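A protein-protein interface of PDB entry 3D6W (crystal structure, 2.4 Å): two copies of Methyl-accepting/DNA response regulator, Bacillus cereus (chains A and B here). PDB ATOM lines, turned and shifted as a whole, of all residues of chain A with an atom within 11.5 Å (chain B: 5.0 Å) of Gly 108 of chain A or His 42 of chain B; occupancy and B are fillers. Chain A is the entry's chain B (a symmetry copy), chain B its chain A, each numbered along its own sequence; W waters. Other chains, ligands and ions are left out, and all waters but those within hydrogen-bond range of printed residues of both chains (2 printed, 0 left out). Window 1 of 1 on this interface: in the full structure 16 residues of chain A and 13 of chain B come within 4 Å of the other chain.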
ATOM      1  N   LYS A  55     -27.230   2.516  -8.906  1.00  0.00           N
ATOM      2  CA  LYS A  55     -25.954   2.238  -8.235  1.00  0.00           C
ATOM      3  C   LYS A  55     -25.802   2.932  -6.899  1.00  0.00           C
ATOM      4  O   LYS A  55     -25.036   2.474  -6.066  1.00  0.00           O
ATOM      5  CB  LYS A  55     -24.793   2.644  -9.168  1.00  0.00           C
ATOM      6  CG  LYS A  55     -24.335   1.459 -10.039  1.00  0.00           C
ATOM      7  CD  LYS A  55     -23.916   1.792 -11.527  1.00  0.00           C
ATOM      8  CE  LYS A  55     -23.886   0.426 -12.425  1.00  0.00           C
ATOM      9  NZ  LYS A  55     -23.496   0.681 -13.874  1.00  0.00           N
ATOM     10  N   ASP A  56     -26.549   4.017  -6.685  1.00  0.00           N
ATOM     11  CA  ASP A  56     -26.571   4.683  -5.387  1.00  0.00           C
ATOM     12  C   ASP A  56     -27.335   3.950  -4.291  1.00  0.00           C
ATOM     13  O   ASP A  56     -27.198   4.291  -3.101  1.00  0.00           O
ATOM     14  CB  ASP A  56     -27.086   6.120  -5.496  1.00  0.00           C
ATOM     15  CG  ASP A  56     -28.587   6.226  -5.834  1.00  0.00           C
ATOM     16  OD1 ASP A  56     -29.163   5.418  -6.571  1.00  0.00           O
ATOM     17  OD2 ASP A  56     -29.196   7.208  -5.364  1.00  0.00           O
ATOM     18  N   ILE A  59     -26.633  -2.725  -4.441  1.00  0.00           N
ATOM     19  CA  ILE A  59     -25.296  -3.238  -4.525  1.00  0.00           C
ATOM     20  C   ILE A  59     -25.272  -4.779  -4.434  1.00  0.00           C
ATOM     21  O   ILE A  59     -25.894  -5.372  -3.561  1.00  0.00           O
ATOM     22  CB  ILE A  59     -24.372  -2.562  -3.455  1.00  0.00           C
ATOM     23  CG1 ILE A  59     -22.953  -3.098  -3.603  1.00  0.00           C
ATOM     24  CG2 ILE A  59     -24.893  -2.761  -2.024  1.00  0.00           C
ATOM     25  CD1 ILE A  59     -21.871  -2.201  -3.012  1.00  0.00           C
ATOM     26  N   VAL A  69     -29.581  -0.779  -0.110  1.00  0.00           N
ATOM     27  CA  VAL A  69     -28.981  -0.177   1.089  1.00  0.00           C
ATOM     28  C   VAL A  69     -29.964   0.627   1.940  1.00  0.00           C
ATOM     29  O   VAL A  69     -29.721   0.861   3.115  1.00  0.00           O
ATOM     30  CB  VAL A  69     -27.720   0.701   0.783  1.00  0.00           C
ATOM     31  CG1 VAL A  69     -26.657  -0.143   0.057  1.00  0.00           C
ATOM     32  CG2 VAL A  69     -28.079   1.964   0.016  1.00  0.00           C
ATOM     33  N   ILE A  72     -31.414  -1.713   4.656  1.00  0.00           N
ATOM     34  CA  ILE A  72     -30.472  -2.249   5.640  1.00  0.00           C
ATOM     35  C   ILE A  72     -30.637  -1.484   6.911  1.00  0.00           C
ATOM     36  O   ILE A  72     -30.528  -0.226   6.897  1.00  0.00           O
ATOM     37  CB  ILE A  72     -29.031  -2.076   5.228  1.00  0.00           C
ATOM     38  CG1 ILE A  72     -28.747  -2.855   3.951  1.00  0.00           C
ATOM     39  CG2 ILE A  72     -28.091  -2.496   6.385  1.00  0.00           C
ATOM     40  CD1 ILE A  72     -27.409  -2.555   3.362  1.00  0.00           C
ATOM     41  N   ILE A  75     -25.382  -3.163   9.871  1.00  0.00           N
ATOM     42  CA  ILE A  75     -24.353  -3.988   9.244  1.00  0.00           C
ATOM     43  C   ILE A  75     -23.481  -4.460  10.390  1.00  0.00           C
ATOM     44  O   ILE A  75     -22.994  -3.627  11.182  1.00  0.00           O
ATOM     45  CB  ILE A  75     -23.416  -3.175   8.292  1.00  0.00           C
ATOM     46  CG1 ILE A  75     -24.194  -2.433   7.193  1.00  0.00           C
ATOM     47  CG2 ILE A  75     -22.327  -4.097   7.692  1.00  0.00           C
ATOM     48  CD1 ILE A  75     -23.440  -1.294   6.507  1.00  0.00           C
ATOM     49  N   PHE A  83     -19.627  -9.793   6.250  1.00  0.00           N
ATOM     50  CA  PHE A  83     -20.634  -9.019   6.995  1.00  0.00           C
ATOM     51  C   PHE A  83     -21.975  -9.702   6.941  1.00  0.00           C
ATOM     52  O   PHE A  83     -22.221 -10.569   6.111  1.00  0.00           O
ATOM     53  CB  PHE A  83     -20.804  -7.592   6.473  1.00  0.00           C
ATOM     54  CG  PHE A  83     -19.519  -6.784   6.451  1.00  0.00           C
ATOM     55  CD1 PHE A  83     -19.037  -6.175   7.610  1.00  0.00           C
ATOM     56  CD2 PHE A  83     -18.804  -6.611   5.270  1.00  0.00           C
ATOM     57  CE1 PHE A  83     -17.866  -5.441   7.590  1.00  0.00           C
ATOM     58  CE2 PHE A  83     -17.644  -5.854   5.254  1.00  0.00           C
ATOM     59  CZ  PHE A  83     -17.181  -5.276   6.414  1.00  0.00           C
ATOM     60  N   LEU A  85     -26.178  -8.470   7.188  1.00  0.00           N
ATOM     61  CA  LEU A  85     -26.989  -7.277   7.069  1.00  0.00           C
ATOM     62  C   LEU A  85     -28.324  -7.567   7.740  1.00  0.00           C
ATOM     63  O   LEU A  85     -29.020  -8.510   7.381  1.00  0.00           O
ATOM     64  CB  LEU A  85     -27.156  -6.865   5.592  1.00  0.00           C
ATOM     65  CG  LEU A  85     -25.875  -6.751   4.767  1.00  0.00           C
ATOM     66  CD1 LEU A  85     -26.159  -6.515   3.323  1.00  0.00           C
ATOM     67  CD2 LEU A  85     -25.031  -5.634   5.287  1.00  0.00           C
ATOM     68  N   TYR A  99     -17.001 -10.267  -1.622  1.00  0.00           N
ATOM     69  CA  TYR A  99     -17.658  -8.979  -1.895  1.00  0.00           C
ATOM     70  C   TYR A  99     -17.458  -7.981  -0.760  1.00  0.00           C
ATOM     71  O   TYR A  99     -17.775  -6.813  -0.944  1.00  0.00           O
ATOM     72  CB  TYR A  99     -19.177  -9.163  -2.161  1.00  0.00           C
ATOM     73  CG  TYR A  99     -19.537  -9.748  -3.526  1.00  0.00           C
ATOM     74  CD1 TYR A  99     -19.545 -11.122  -3.733  1.00  0.00           C
ATOM     75  CD2 TYR A  99     -19.877  -8.920  -4.603  1.00  0.00           C
ATOM     76  CE1 TYR A  99     -19.875 -11.653  -4.956  1.00  0.00           C
ATOM     77  CE2 TYR A  99     -20.209  -9.443  -5.828  1.00  0.00           C
ATOM     78  CZ  TYR A  99     -20.213 -10.807  -6.006  1.00  0.00           C
ATOM     79  OH  TYR A  99     -20.522 -11.354  -7.236  1.00  0.00           O
ATOM     80  N   ALA A 100     -16.932  -8.441   0.383  1.00  0.00           N
ATOM     81  CA  ALA A 100     -16.858  -7.650   1.616  1.00  0.00           C
ATOM     82  C   ALA A 100     -16.053  -6.365   1.463  1.00  0.00           C
ATOM     83  O   ALA A 100     -16.358  -5.335   2.073  1.00  0.00           O
ATOM     84  CB  ALA A 100     -16.278  -8.492   2.729  1.00  0.00           C
ATOM     85  N   SER A 101     -15.029  -6.428   0.632  1.00  0.00           N
ATOM     86  CA  SER A 101     -14.132  -5.312   0.433  1.00  0.00           C
ATOM     87  C   SER A 101     -14.789  -4.265  -0.469  1.00  0.00           C
ATOM     88  O   SER A 101     -14.838  -3.083  -0.138  1.00  0.00           O
ATOM     89  CB  SER A 101     -12.815  -5.836  -0.159  1.00  0.00           C
ATOM     90  OG  SER A 101     -11.871  -4.810  -0.295  1.00  0.00           O
ATOM     91  N   TYR A 102     -15.296  -4.710  -1.611  1.00  0.00           N
ATOM     92  CA  TYR A 102     -16.112  -3.884  -2.512  1.00  0.00           C
ATOM     93  C   TYR A 102     -17.292  -3.262  -1.782  1.00  0.00           C
ATOM     94  O   TYR A 102     -17.575  -2.079  -1.921  1.00  0.00           O
ATOM     95  CB  TYR A 102     -16.619  -4.794  -3.631  1.00  0.00           C
ATOM     96  CG  TYR A 102     -17.637  -4.234  -4.612  1.00  0.00           C
ATOM     97  CD1 TYR A 102     -17.250  -3.366  -5.650  1.00  0.00           C
ATOM     98  CD2 TYR A 102     -18.970  -4.656  -4.563  1.00  0.00           C
ATOM     99  CE1 TYR A 102     -18.190  -2.893  -6.577  1.00  0.00           C
ATOM    100  CE2 TYR A 102     -19.887  -4.203  -5.464  1.00  0.00           C
ATOM    101  CZ  TYR A 102     -19.505  -3.335  -6.473  1.00  0.00           C
ATOM    102  OH  TYR A 102     -20.459  -2.902  -7.355  1.00  0.00           O
ATOM    103  N   PHE A 103     -17.989  -4.072  -0.993  1.00  0.00           N
ATOM    104  CA  PHE A 103     -19.133  -3.614  -0.224  1.00  0.00           C
ATOM    105  C   PHE A 103     -18.779  -2.467   0.685  1.00  0.00           C
ATOM    106  O   PHE A 103     -19.453  -1.445   0.660  1.00  0.00           O
ATOM    107  CB  PHE A 103     -19.696  -4.754   0.607  1.00  0.00           C
ATOM    108  CG  PHE A 103     -20.957  -4.403   1.345  1.00  0.00           C
ATOM    109  CD1 PHE A 103     -22.174  -4.361   0.678  1.00  0.00           C
ATOM    110  CD2 PHE A 103     -20.923  -4.125   2.708  1.00  0.00           C
ATOM    111  CE1 PHE A 103     -23.332  -4.027   1.345  1.00  0.00           C
ATOM    112  CE2 PHE A 103     -22.057  -3.810   3.385  1.00  0.00           C
ATOM    113  CZ  PHE A 103     -23.292  -3.753   2.695  1.00  0.00           C
ATOM    114  N   ARG A 104     -17.724  -2.610   1.493  1.00  0.00           N
ATOM    115  CA  ARG A 104     -17.369  -1.532   2.419  1.00  0.00           C
ATOM    116  C   ARG A 104     -16.741  -0.317   1.740  1.00  0.00           C
ATOM    117  O   ARG A 104     -16.918   0.812   2.232  1.00  0.00           O
ATOM    118  CB  ARG A 104     -16.487  -2.025   3.559  1.00  0.00           C
ATOM    119  CG  ARG A 104     -15.020  -2.145   3.246  1.00  0.00           C
ATOM    120  CD  ARG A 104     -14.289  -2.804   4.396  1.00  0.00           C
ATOM    121  NE  ARG A 104     -14.445  -2.032   5.628  1.00  0.00           N
ATOM    122  CZ  ARG A 104     -14.297  -2.516   6.853  1.00  0.00           C
ATOM    123  NH1 ARG A 104     -13.972  -3.785   7.030  1.00  0.00           N
ATOM    124  NH2 ARG A 104     -14.474  -1.730   7.903  1.00  0.00           N
ATOM    125  N   LYS A 105     -15.996  -0.530   0.642  1.00  0.00           N
ATOM    126  CA  LYS A 105     -15.466   0.610  -0.112  1.00  0.00           C
ATOM    127  C   LYS A 105     -16.621   1.473  -0.589  1.00  0.00           C
ATOM    128  O   LYS A 105     -16.616   2.678  -0.380  1.00  0.00           O
ATOM    129  CB  LYS A 105     -14.578   0.201  -1.306  1.00  0.00           C
ATOM    130  CG  LYS A 105     -13.269  -0.470  -0.898  1.00  0.00           C
ATOM    131  CD  LYS A 105     -12.169  -0.365  -1.983  1.00  0.00           C
ATOM    132  CE  LYS A 105     -11.226  -1.574  -1.991  1.00  0.00           C
ATOM    133  NZ  LYS A 105      -9.853  -1.285  -1.462  1.00  0.00           N
ATOM    134  N   LEU A 106     -17.625   0.847  -1.195  1.00  0.00           N
ATOM    135  CA  LEU A 106     -18.802   1.575  -1.728  1.00  0.00           C
ATOM    136  C   LEU A 106     -19.660   2.267  -0.664  1.00  0.00           C
ATOM    137  O   LEU A 106     -20.164   3.376  -0.886  1.00  0.00           O
ATOM    138  CB  LEU A 106     -19.691   0.641  -2.582  1.00  0.00           C
ATOM    139  CG  LEU A 106     -19.384   0.685  -4.078  1.00  0.00           C
ATOM    140  CD1 LEU A 106     -17.915   0.326  -4.476  1.00  0.00           C
ATOM    141  CD2 LEU A 106     -20.404  -0.181  -4.803  1.00  0.00           C
ATOM    142  N   LEU A 107     -19.841   1.603   0.480  1.00  0.00           N
ATOM    143  CA  LEU A 107     -20.612   2.181   1.594  1.00  0.00           C
ATOM    144  C   LEU A 107     -19.785   3.105   2.494  1.00  0.00           C
ATOM    145  O   LEU A 107     -20.343   3.782   3.368  1.00  0.00           O
ATOM    146  CB  LEU A 107     -21.301   1.085   2.413  1.00  0.00           C
ATOM    147  CG  LEU A 107     -22.633   0.677   1.788  1.00  0.00           C
ATOM    148  CD1 LEU A 107     -22.461  -0.628   1.095  1.00  0.00           C
ATOM    149  CD2 LEU A 107     -23.761   0.556   2.815  1.00  0.00           C
ATOM    150  N   GLY A 108     -18.472   3.118   2.281  1.00  0.00           N
ATOM    151  CA  GLY A 108     -17.561   4.048   2.944  1.00  0.00           C
ATOM    152  C   GLY A 108     -17.261   3.858   4.424  1.00  0.00           C
ATOM    153  O   GLY A 108     -17.106   4.839   5.156  1.00  0.00           O
ATOM    154  N   PHE A 109     -17.185   2.612   4.879  1.00  0.00           N
ATOM    155  CA  PHE A 109     -16.648   2.312   6.212  1.00  0.00           C
ATOM    156  C   PHE A 109     -15.387   1.423   6.057  1.00  0.00           C
ATOM    157  O   PHE A 109     -15.224   0.736   5.062  1.00  0.00           O
ATOM    158  CB  PHE A 109     -17.730   1.754   7.150  1.00  0.00           C
ATOM    159  CG  PHE A 109     -18.344   0.452   6.695  1.00  0.00           C
ATOM    160  CD1 PHE A 109     -18.005  -0.747   7.318  1.00  0.00           C
ATOM    161  CD2 PHE A 109     -19.274   0.427   5.685  1.00  0.00           C
ATOM    162  CE1 PHE A 109     -18.571  -1.928   6.912  1.00  0.00           C
ATOM    163  CE2 PHE A 109     -19.837  -0.762   5.264  1.00  0.00           C
ATOM    164  CZ  PHE A 109     -19.499  -1.930   5.875  1.00  0.00           C
ATOM    165  N   GLY A 110     -14.455   1.521   6.992  1.00  0.00           N
ATOM    166  CA  GLY A 110     -13.046   1.049   6.761  1.00  0.00           C
ATOM    167  C   GLY A 110     -12.008   1.909   7.424  1.00  0.00           C
ATOM    168  O   GLY A 110     -11.416   1.526   8.438  1.00  0.00           O
ATOM    169  N   VAL B   5     -24.961   7.533   4.137  1.00  0.00           N
ATOM    170  CA  VAL B   5     -23.725   7.616   4.916  1.00  0.00           C
ATOM    171  C   VAL B   5     -23.772   6.504   5.979  1.00  0.00           C
ATOM    172  O   VAL B   5     -24.793   6.336   6.652  1.00  0.00           O
ATOM    173  CB  VAL B   5     -23.564   8.955   5.660  1.00  0.00           C
ATOM    174  CG1 VAL B   5     -22.056   9.229   5.934  1.00  0.00           C
ATOM    175  CG2 VAL B   5     -24.193  10.090   4.889  1.00  0.00           C
ATOM    176  N   THR B   6     -22.678   5.742   6.096  1.00  0.00           N
ATOM    177  CA  THR B   6     -22.575   4.649   7.070  1.00  0.00           C
ATOM    178  C   THR B   6     -21.885   5.198   8.302  1.00  0.00           C
ATOM    179  O   THR B   6     -20.726   5.595   8.247  1.00  0.00           O
ATOM    180  CB  THR B   6     -21.901   3.404   6.489  1.00  0.00           C
ATOM    181  OG1 THR B   6     -22.560   3.048   5.255  1.00  0.00           O
ATOM    182  CG2 THR B   6     -22.023   2.226   7.443  1.00  0.00           C
ATOM    183  N   THR B  31     -14.828  12.604  12.628  1.00  0.00           N
ATOM    184  CA  THR B  31     -16.076  13.158  12.083  1.00  0.00           C
ATOM    185  C   THR B  31     -17.284  12.480  12.679  1.00  0.00           C
ATOM    186  O   THR B  31     -17.412  11.282  12.615  1.00  0.00           O
ATOM    187  CB  THR B  31     -16.156  13.008  10.554  1.00  0.00           C
ATOM    188  OG1 THR B  31     -15.041  13.682   9.999  1.00  0.00           O
ATOM    189  CG2 THR B  31     -17.463  13.598   9.983  1.00  0.00           C
ATOM    190  N   VAL B  33     -21.225  12.141  12.364  1.00  0.00           N
ATOM    191  CA  VAL B  33     -22.404  12.311  11.541  1.00  0.00           C
ATOM    192  C   VAL B  33     -23.627  12.248  12.473  1.00  0.00           C
ATOM    193  O   VAL B  33     -23.918  11.217  13.081  1.00  0.00           O
ATOM    194  CB  VAL B  33     -22.450  11.237  10.415  1.00  0.00           C
ATOM    195  CG1 VAL B  33     -23.499  11.595   9.389  1.00  0.00           C
ATOM    196  CG2 VAL B  33     -21.091  11.110   9.733  1.00  0.00           C
ATOM    197  N   GLY B  40     -22.959   8.939  14.947  1.00  0.00           N
ATOM    198  CA  GLY B  40     -21.958   7.943  14.712  1.00  0.00           C
ATOM    199  C   GLY B  40     -20.773   8.565  14.041  1.00  0.00           C
ATOM    200  O   GLY B  40     -20.773   9.723  13.684  1.00  0.00           O
ATOM    201  N   THR B  41     -19.773   7.742  13.855  1.00  0.00           N
ATOM    202  CA  THR B  41     -18.461   8.163  13.466  1.00  0.00           C
ATOM    203  C   THR B  41     -18.304   7.788  11.975  1.00  0.00           C
ATOM    204  O   THR B  41     -18.910   6.814  11.489  1.00  0.00           O
ATOM    205  CB  THR B  41     -17.474   7.480  14.430  1.00  0.00           C
ATOM    206  OG1 THR B  41     -17.066   8.438  15.415  1.00  0.00           O
ATOM    207  CG2 THR B  41     -16.288   6.881  13.730  1.00  0.00           C
ATOM    208  N   HIS B  42     -17.547   8.606  11.254  1.00  0.00           N
ATOM    209  CA  HIS B  42     -17.198   8.321   9.896  1.00  0.00           C
ATOM    210  C   HIS B  42     -15.734   8.620   9.707  1.00  0.00           C
ATOM    211  O   HIS B  42     -15.211   9.542  10.322  1.00  0.00           O
ATOM    212  CB  HIS B  42     -18.020   9.148   8.900  1.00  0.00           C
ATOM    213  CG  HIS B  42     -18.043   8.536   7.534  1.00  0.00           C
ATOM    214  ND1 HIS B  42     -16.959   8.573   6.686  1.00  0.00           N
ATOM    215  CD2 HIS B  42     -18.982   7.793   6.904  1.00  0.00           C
ATOM    216  CE1 HIS B  42     -17.234   7.899   5.581  1.00  0.00           C
ATOM    217  NE2 HIS B  42     -18.460   7.421   5.683  1.00  0.00           N
ATOM    218  N   LYS B  43     -15.085   7.868   8.823  1.00  0.00           N
ATOM    219  CA  LYS B  43     -13.664   8.048   8.573  1.00  0.00           C
ATOM    220  C   LYS B  43     -13.305   9.231   7.672  1.00  0.00           C
ATOM    221  O   LYS B  43     -12.164   9.668   7.654  1.00  0.00           O
ATOM    222  CB  LYS B  43     -13.061   6.743   8.016  1.00  0.00           C
ATOM    223  CG  LYS B  43     -13.668   6.231   6.693  1.00  0.00           C
ATOM    224  CD  LYS B  43     -12.830   5.102   6.126  1.00  0.00           C
ATOM    225  CE  LYS B  43     -13.140   4.883   4.665  1.00  0.00           C
ATOM    226  NZ  LYS B  43     -12.687   3.525   4.265  1.00  0.00           N
ATOM    227  N   TYR B  44     -14.244   9.753   6.906  1.00  0.00           N
ATOM    228  CA  TYR B  44     -13.925  10.853   5.990  1.00  0.00           C
ATOM    229  C   TYR B  44     -13.901  12.155   6.722  1.00  0.00           C
ATOM    230  O   TYR B  44     -14.589  12.327   7.712  1.00  0.00           O
ATOM    231  CB  TYR B  44     -14.939  10.993   4.855  1.00  0.00           C
ATOM    232  CG  TYR B  44     -15.014   9.878   3.864  1.00  0.00           C
ATOM    233  CD1 TYR B  44     -14.006   8.936   3.727  1.00  0.00           C
ATOM    234  CD2 TYR B  44     -16.115   9.776   3.038  1.00  0.00           C
ATOM    235  CE1 TYR B  44     -14.114   7.908   2.814  1.00  0.00           C
ATOM    236  CE2 TYR B  44     -16.227   8.745   2.115  1.00  0.00           C
ATOM    237  CZ  TYR B  44     -15.230   7.828   2.013  1.00  0.00           C
ATOM    238  OH  TYR B  44     -15.377   6.828   1.100  1.00  0.00           O
ATOM    239  N   PHE B  49     -16.233  14.970   2.807  1.00  0.00           N
ATOM    240  CA  PHE B  49     -17.685  15.110   2.764  1.00  0.00           C
ATOM    241  C   PHE B  49     -18.166  16.296   1.925  1.00  0.00           C
ATOM    242  O   PHE B  49     -19.196  16.200   1.288  1.00  0.00           O
ATOM    243  CB  PHE B  49     -18.281  15.185   4.177  1.00  0.00           C
ATOM    244  CG  PHE B  49     -18.555  13.852   4.786  1.00  0.00           C
ATOM    245  CD1 PHE B  49     -19.559  13.053   4.295  1.00  0.00           C
ATOM    246  CD2 PHE B  49     -17.818  13.398   5.857  1.00  0.00           C
ATOM    247  CE1 PHE B  49     -19.828  11.805   4.864  1.00  0.00           C
ATOM    248  CE2 PHE B  49     -18.085  12.168   6.428  1.00  0.00           C
ATOM    249  CZ  PHE B  49     -19.091  11.377   5.931  1.00  0.00           C
HETATM  250  O   HOH W   1     -16.685   5.343   7.911  1.00  0.00           O
HETATM  251  O   HOH W   2     -20.589   6.387   4.119  1.00  0.00           O
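NE of Arg 104 of chain A lies within hydrogen-bond range of O of Phe 109 of chain A (2.9 Å). The backbone carbonyl oxygen of Thr 31 of chain B sits at hydrogen-bond distance from the backbone NH of His 42 of chain B (3.0 Å). OG1 of Thr 31 of chain B lies within hydrogen-bond range of O of Tyr 44 of chain B, 2.7 Å away. A ring nitrogen (ND1) of His 42 of chain B is in hydrogen-bond range of the backbone NH (N) of Tyr 44 of chain B, at 3.0 Å.
Water W2 lies within hydrogen-bond range of O of Leu 107 of chain A (2.7 Å), NE2 of His 42 of chain B (2.8 Å) and N of Thr 6 of chain B (2.9 Å). Water W1 lies within hydrogen-bond range of O of Gly 108 of chain A (2.8 Å), N of Lys 43 of chain B (3.1 Å) and ND1 of His 42 of chain B (3.5 Å).
The backbone carbonyl oxygen (O) of Gly 108 of chain A sits at hydrogen-bond distance from a ring nitrogen (NE2) of His 42 of chain B (3.0 Å). The side-chain hydroxyl of Thr 6 of chain B lies within hydrogen-bond range of the backbone carbonyl oxygen of Leu 107 of chain A (3.0 Å).
Hydrophobic or aromatic side chains of chain A within 4 Å of the printed part of chain B: Ile 75, Leu 107 and Phe 109. Among the printed residues, no Asp or Glu carboxylate lies within 4 Å of a Lys or Arg side-chain nitrogen of the other chain.
No position is printed for both chains. Of the 8 pairs that touch across the chains among the printed residues, none has its exchanged pair printed and touching as well.
Ile 75 of chain A touches Thr 6 of chain B. Gly 108 of chain A touches Lys 43 of chain B (O to CE, 3.997 Å). Tyr 44 of chain B touches Gly 108 of chain A (OH to CA, 3.99 Å). CG2 of Thr 6 of chain B touches CD2 of Phe 109 of chain A, at 3.7 Å. Phe 109 of chain A touches Lys 43 of chain B. Lys 43 of chain B touches Gly 110 of chain A (NZ to CA, 3.5 Å).
Printed residues of chain B within 4 Å of Gly 108 of chain A: His 42, Lys 43 and Tyr 44. His 42 of chain B touches just one residue of chain A: Gly 108 (3.0 Å). No residue of chain A comes within 4 Å of Val 5 of chain B. Thr 31 of chain B touches none of the printed residues of chain A. No residue of chain A comes within 4 Å of Val 33 of chain B. Gly 40 of chain B touches none of the printed residues of chain A. No residue of chain A comes within 4 Å of Thr 41 of chain B. Printed residues of chain B within 4 Å of Ile 75 of chain A: Thr 6. Of the printed residues of chain A, Tyr 44 of chain B touches Gly 108. Lys 55 of chain A touches none of the printed residues of chain B. The nearest printed residue of chain B that does not touch Gly 108 of chain A is Thr 6 of chain B (4.8 Å). The nearest residue of chain A that does not touch His 42 of chain B is Leu 107 of chain A (4.7 Å).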
